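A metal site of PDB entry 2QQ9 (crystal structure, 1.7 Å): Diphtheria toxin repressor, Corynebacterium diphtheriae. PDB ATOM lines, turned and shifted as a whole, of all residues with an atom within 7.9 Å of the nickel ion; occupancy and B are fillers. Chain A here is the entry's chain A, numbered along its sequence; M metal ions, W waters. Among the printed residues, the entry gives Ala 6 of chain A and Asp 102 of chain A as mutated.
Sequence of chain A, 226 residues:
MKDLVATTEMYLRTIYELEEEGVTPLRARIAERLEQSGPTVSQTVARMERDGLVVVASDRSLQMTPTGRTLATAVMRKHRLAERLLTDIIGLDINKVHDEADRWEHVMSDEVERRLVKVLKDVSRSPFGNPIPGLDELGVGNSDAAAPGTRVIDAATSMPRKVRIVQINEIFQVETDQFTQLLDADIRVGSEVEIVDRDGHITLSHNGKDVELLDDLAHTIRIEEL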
ATOM      1  N   ALA A   6      24.325   5.081  16.234  1.00  0.00           N
ATOM      2  CA  ALA A   6      23.993   4.005  17.221  1.00  0.00           C
ATOM      3  C   ALA A   6      22.532   3.582  17.133  1.00  0.00           C
ATOM      4  O   ALA A   6      22.186   2.400  17.255  1.00  0.00           O
ATOM      5  CB  ALA A   6      24.308   4.456  18.659  1.00  0.00           C
ATOM      6  N   THR A   7      21.681   4.598  16.945  1.00  0.00           N
ATOM      7  CA  THR A   7      20.231   4.397  16.761  1.00  0.00           C
ATOM      8  C   THR A   7      19.959   3.507  15.514  1.00  0.00           C
ATOM      9  O   THR A   7      19.297   2.498  15.611  1.00  0.00           O
ATOM     10  CB  THR A   7      19.467   5.732  16.724  1.00  0.00           C
ATOM     11  OG1 THR A   7      19.507   6.366  18.014  1.00  0.00           O
ATOM     12  CG2 THR A   7      17.997   5.503  16.335  1.00  0.00           C
ATOM     13  N   GLU A   9      22.013   1.576  13.886  1.00  0.00           N
ATOM     14  CA  GLU A   9      22.524   0.221  14.152  1.00  0.00           C
ATOM     15  C   GLU A   9      21.578  -0.594  15.053  1.00  0.00           C
ATOM     16  O   GLU A   9      21.466  -1.827  14.937  1.00  0.00           O
ATOM     17  CB  GLU A   9      23.906   0.339  14.814  1.00  0.00           C
ATOM     18  CG  GLU A   9      24.963   0.973  13.891  1.00  0.00           C
ATOM     19  CD  GLU A   9      26.391   0.965  14.537  1.00  0.00           C
ATOM     20  OE1 GLU A   9      26.485   0.806  15.752  1.00  0.00           O
ATOM     21  OE2 GLU A   9      27.376   1.188  13.828  1.00  0.00           O
ATOM     22  N   MET A  10      20.914   0.085  15.995  1.00  0.00           N
ATOM     23  CA  MET A  10      20.065  -0.641  16.929  1.00  0.00           C
ATOM     24  C   MET A  10      18.820  -1.114  16.156  1.00  0.00           C
ATOM     25  O   MET A  10      18.427  -2.279  16.312  1.00  0.00           O
ATOM     26  CB  MET A  10      19.658   0.212  18.169  1.00  0.00           C
ATOM     27  CG  MET A  10      20.793   0.338  19.178  1.00  0.00           C
ATOM     28  SD  MET A  10      21.150  -1.355  19.827  1.00  0.00           S
ATOM     29  CE  MET A  10      19.646  -1.749  20.796  1.00  0.00           C
ATOM     30  N   TYR A  11      18.268  -0.233  15.331  1.00  0.00           N
ATOM     31  CA  TYR A  11      17.124  -0.632  14.482  1.00  0.00           C
ATOM     32  C   TYR A  11      17.531  -1.830  13.610  1.00  0.00           C
ATOM     33  O   TYR A  11      16.835  -2.828  13.550  1.00  0.00           O
ATOM     34  CB  TYR A  11      16.660   0.524  13.622  1.00  0.00           C
ATOM     35  CG  TYR A  11      15.803   1.515  14.391  1.00  0.00           C
ATOM     36  CD1 TYR A  11      16.214   2.032  15.627  1.00  0.00           C
ATOM     37  CD2 TYR A  11      14.572   1.920  13.867  1.00  0.00           C
ATOM     38  CE1 TYR A  11      15.417   2.927  16.348  1.00  0.00           C
ATOM     39  CE2 TYR A  11      13.775   2.831  14.545  1.00  0.00           C
ATOM     40  CZ  TYR A  11      14.201   3.326  15.813  1.00  0.00           C
ATOM     41  OH  TYR A  11      13.359   4.227  16.435  1.00  0.00           O
ATOM     42  N   ARG A  13      20.032  -4.072  14.108  1.00  0.00           N
ATOM     43  CA  ARG A  13      20.286  -5.318  14.851  1.00  0.00           C
ATOM     44  C   ARG A  13      18.933  -5.904  15.275  1.00  0.00           C
ATOM     45  O   ARG A  13      18.708  -7.129  15.265  1.00  0.00           O
ATOM     46  CB  ARG A  13      21.167  -5.034  16.086  1.00  0.00           C
ATOM     47  CG  ARG A  13      21.919  -6.278  16.467  1.00  0.00           C
ATOM     48  CD  ARG A  13      21.734  -6.699  17.872  1.00  0.00           C
ATOM     49  NE  ARG A  13      21.886  -5.695  18.952  1.00  0.00           N
ATOM     50  CZ  ARG A  13      21.197  -5.702  20.081  1.00  0.00           C
ATOM     51  NH1 ARG A  13      20.188  -6.585  20.311  1.00  0.00           N
ATOM     52  NH2 ARG A  13      21.416  -4.738  20.989  1.00  0.00           N
ATOM     53  N   LEU A  34      12.575  -2.171  21.365  1.00  0.00           N
ATOM     54  CA  LEU A  34      13.412  -1.052  21.751  1.00  0.00           C
ATOM     55  C   LEU A  34      12.749  -0.104  22.770  1.00  0.00           C
ATOM     56  O   LEU A  34      13.362   0.896  23.193  1.00  0.00           O
ATOM     57  CB  LEU A  34      13.857  -0.267  20.517  1.00  0.00           C
ATOM     58  CG  LEU A  34      14.681  -1.026  19.465  1.00  0.00           C
ATOM     59  CD1 LEU A  34      14.920  -0.115  18.256  1.00  0.00           C
ATOM     60  CD2 LEU A  34      15.970  -1.498  20.048  1.00  0.00           C
ATOM     61  N   VAL A  75      26.978  -5.226  13.312  1.00  0.00           N
ATOM     62  CA  VAL A  75      26.549  -4.807  14.634  1.00  0.00           C
ATOM     63  C   VAL A  75      26.261  -6.096  15.436  1.00  0.00           C
ATOM     64  O   VAL A  75      26.687  -6.223  16.575  1.00  0.00           O
ATOM     65  CB  VAL A  75      25.278  -3.932  14.525  1.00  0.00           C
ATOM     66  CG1 VAL A  75      24.747  -3.635  15.945  1.00  0.00           C
ATOM     67  CG2 VAL A  75      25.588  -2.654  13.794  1.00  0.00           C
ATOM     68  N   HIS A  79      28.321  -7.183  18.720  1.00  0.00           N
ATOM     69  CA  HIS A  79      27.512  -7.363  19.914  1.00  0.00           C
ATOM     70  C   HIS A  79      27.866  -8.710  20.544  1.00  0.00           C
ATOM     71  O   HIS A  79      28.248  -8.781  21.683  1.00  0.00           O
ATOM     72  CB  HIS A  79      26.016  -7.333  19.587  1.00  0.00           C
ATOM     73  CG  HIS A  79      25.177  -7.472  20.805  1.00  0.00           C
ATOM     74  ND1 HIS A  79      25.063  -6.484  21.760  1.00  0.00           N
ATOM     75  CD2 HIS A  79      24.394  -8.511  21.229  1.00  0.00           C
ATOM     76  CE1 HIS A  79      24.227  -6.895  22.714  1.00  0.00           C
ATOM     77  NE2 HIS A  79      23.834  -8.124  22.424  1.00  0.00           N
ATOM     78  N   HIS A  98      24.587  -8.626  28.468  1.00  0.00           N
ATOM     79  CA  HIS A  98      23.833  -8.077  27.322  1.00  0.00           C
ATOM     80  C   HIS A  98      23.796  -6.527  27.287  1.00  0.00           C
ATOM     81  O   HIS A  98      24.094  -5.917  26.276  1.00  0.00           O
ATOM     82  CB  HIS A  98      22.420  -8.681  27.127  1.00  0.00           C
ATOM     83  CG  HIS A  98      21.647  -7.918  26.112  1.00  0.00           C
ATOM     84  ND1 HIS A  98      21.901  -8.033  24.770  1.00  0.00           N
ATOM     85  CD2 HIS A  98      20.767  -6.890  26.249  1.00  0.00           C
ATOM     86  CE1 HIS A  98      21.191  -7.154  24.100  1.00  0.00           C
ATOM     87  NE2 HIS A  98      20.489  -6.430  24.967  1.00  0.00           N
ATOM     88  N   ASP A  99      23.489  -5.913  28.431  1.00  0.00           N
ATOM     89  CA  ASP A  99      23.254  -4.482  28.486  1.00  0.00           C
ATOM     90  C   ASP A  99      24.567  -3.795  28.185  1.00  0.00           C
ATOM     91  O   ASP A  99      24.637  -2.818  27.420  1.00  0.00           O
ATOM     92  CB  ASP A  99      22.716  -4.104  29.891  1.00  0.00           C
ATOM     93  CG  ASP A  99      21.172  -4.267  30.036  1.00  0.00           C
ATOM     94  OD1 ASP A  99      20.443  -4.467  29.037  1.00  0.00           O
ATOM     95  OD2 ASP A  99      20.666  -4.130  31.184  1.00  0.00           O
ATOM     96  N   GLU A 100      25.633  -4.351  28.737  1.00  0.00           N
ATOM     97  CA  GLU A 100      26.941  -3.756  28.458  1.00  0.00           C
ATOM     98  C   GLU A 100      27.280  -3.832  26.964  1.00  0.00           C
ATOM     99  O   GLU A 100      27.626  -2.816  26.344  1.00  0.00           O
ATOM    100  CB  GLU A 100      28.045  -4.416  29.307  1.00  0.00           C
ATOM    101  CG  GLU A 100      29.341  -3.639  29.274  1.00  0.00           C
ATOM    102  CD  GLU A 100      29.439  -2.617  30.376  1.00  0.00           C
ATOM    103  OE1 GLU A 100      28.698  -2.789  31.375  1.00  0.00           O
ATOM    104  OE2 GLU A 100      30.272  -1.710  30.247  1.00  0.00           O
ATOM    105  N   ALA A 101      27.035  -5.021  26.380  1.00  0.00           N
ATOM    106  CA  ALA A 101      27.318  -5.236  24.950  1.00  0.00           C
ATOM    107  C   ALA A 101      26.402  -4.403  24.059  1.00  0.00           C
ATOM    108  O   ALA A 101      26.766  -4.112  22.892  1.00  0.00           O
ATOM    109  CB  ALA A 101      27.217  -6.649  24.605  1.00  0.00           C
ATOM    110  N   ASP A 102      25.266  -4.021  24.611  1.00  0.00           N
ATOM    111  CA  ASP A 102      24.271  -3.205  23.939  1.00  0.00           C
ATOM    112  C   ASP A 102      24.938  -1.846  23.689  1.00  0.00           C
ATOM    113  O   ASP A 102      24.740  -1.192  22.649  1.00  0.00           O
ATOM    114  CB  ASP A 102      22.970  -3.080  24.782  1.00  0.00           C
ATOM    115  CG  ASP A 102      21.745  -2.504  23.987  1.00  0.00           C
ATOM    116  OD1 ASP A 102      21.830  -2.248  22.756  1.00  0.00           O
ATOM    117  OD2 ASP A 102      20.701  -2.404  24.612  1.00  0.00           O
ATOM    118  N   ARG A 103      25.805  -1.433  24.630  1.00  0.00           N
ATOM    119  CA  ARG A 103      26.544  -0.211  24.389  1.00  0.00           C
ATOM    120  C   ARG A 103      27.805  -0.406  23.543  1.00  0.00           C
ATOM    121  O   ARG A 103      28.068   0.387  22.621  1.00  0.00           O
ATOM    122  CB  ARG A 103      26.916   0.476  25.716  1.00  0.00           C
ATOM    123  CG  ARG A 103      25.687   0.960  26.514  1.00  0.00           C
ATOM    124  CD  ARG A 103      26.041   1.899  27.637  1.00  0.00           C
ATOM    125  NE  ARG A 103      26.970   1.283  28.578  1.00  0.00           N
ATOM    126  CZ  ARG A 103      26.623   0.384  29.475  1.00  0.00           C
ATOM    127  NH1 ARG A 103      25.346  -0.059  29.560  1.00  0.00           N
ATOM    128  NH2 ARG A 103      27.580  -0.117  30.273  1.00  0.00           N
ATOM    129  N   TRP A 104      28.576  -1.460  23.837  1.00  0.00           N
ATOM    130  CA  TRP A 104      29.879  -1.621  23.242  1.00  0.00           C
ATOM    131  C   TRP A 104      29.828  -1.977  21.727  1.00  0.00           C
ATOM    132  O   TRP A 104      30.752  -1.700  20.961  1.00  0.00           O
ATOM    133  CB  TRP A 104      30.608  -2.693  23.998  1.00  0.00           C
ATOM    134  CG  TRP A 104      31.004  -2.367  25.380  1.00  0.00           C
ATOM    135  CD1 TRP A 104      30.438  -1.486  26.266  1.00  0.00           C
ATOM    136  CD2 TRP A 104      32.124  -2.940  26.032  1.00  0.00           C
ATOM    137  NE1 TRP A 104      31.164  -1.518  27.467  1.00  0.00           N
ATOM    138  CE2 TRP A 104      32.193  -2.385  27.348  1.00  0.00           C
ATOM    139  CE3 TRP A 104      33.080  -3.867  25.631  1.00  0.00           C
ATOM    140  CZ2 TRP A 104      33.209  -2.747  28.262  1.00  0.00           C
ATOM    141  CZ3 TRP A 104      34.075  -4.239  26.541  1.00  0.00           C
ATOM    142  CH2 TRP A 104      34.102  -3.688  27.853  1.00  0.00           C
ATOM    143  N   GLU A 105      28.735  -2.639  21.363  1.00  0.00           N
ATOM    144  CA  GLU A 105      28.486  -2.971  19.955  1.00  0.00           C
ATOM    145  C   GLU A 105      28.593  -1.761  18.946  1.00  0.00           C
ATOM    146  O   GLU A 105      28.923  -1.967  17.752  1.00  0.00           O
ATOM    147  CB  GLU A 105      27.153  -3.702  19.808  1.00  0.00           C
ATOM    148  CG  GLU A 105      25.910  -2.746  20.050  1.00  0.00           C
ATOM    149  CD  GLU A 105      24.587  -3.484  19.922  1.00  0.00           C
ATOM    150  OE1 GLU A 105      24.492  -4.516  19.216  1.00  0.00           O
ATOM    151  OE2 GLU A 105      23.650  -3.040  20.520  1.00  0.00           O
ATOM    152  N   HIS A 106      28.386  -0.536  19.478  1.00  0.00           N
ATOM    153  CA  HIS A 106      28.367   0.649  18.592  1.00  0.00           C
ATOM    154  C   HIS A 106      29.717   1.326  18.523  1.00  0.00           C
ATOM    155  O   HIS A 106      29.880   2.256  17.767  1.00  0.00           O
ATOM    156  CB  HIS A 106      27.314   1.627  19.064  1.00  0.00           C
ATOM    157  CG  HIS A 106      25.963   0.993  19.180  1.00  0.00           C
ATOM    158  ND1 HIS A 106      25.257   0.516  18.086  1.00  0.00           N
ATOM    159  CD2 HIS A 106      25.255   0.634  20.282  1.00  0.00           C
ATOM    160  CE1 HIS A 106      24.143  -0.061  18.515  1.00  0.00           C
ATOM    161  NE2 HIS A 106      24.090   0.031  19.825  1.00  0.00           N
HETATM  162 NI    NI M   1      23.058  -1.175  21.299  1.00  0.00          NI
HETATM  163  O   HOH W   1      22.226   0.778  22.254  1.00  0.00           O
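The guanidinium group (NE) of Arg 13 lies within salt-bridge range of the side-chain carboxylate (OE1) of Glu 105, at 2.9 Å.
The side-chain carboxylate (OE1) of Glu 105 sits close to a ring nitrogen (ND1) of His 79 (3.3 Å).
OD1 of Asp 102 lies close to NH2 of Arg 13, at 3.1 Å.
ND1 of His 106 sits at hydrogen-bond distance from OE1 of Glu 9 (2.7 Å).
SD of Met 10 lies close to NH2 of Arg 13 (3.6 Å).
Arg 13 touches the nickel ion.
The nearest printed residue that does not touch the nickel ion is Arg 103 (4.3 Å).
The nickel ion is bound by the side-chain carboxylate of Glu 105 (2.1 Å), the backbone carbonyl oxygen of Asp 102 (2.2 Å), a ring nitrogen (NE2) of His 106 (2.2 Å), the side-chain carboxylate of Asp 102 (2.2 Å), water W1 (2.3 Å) and the side-chain sulfur of Met 10 (2.4 Å).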
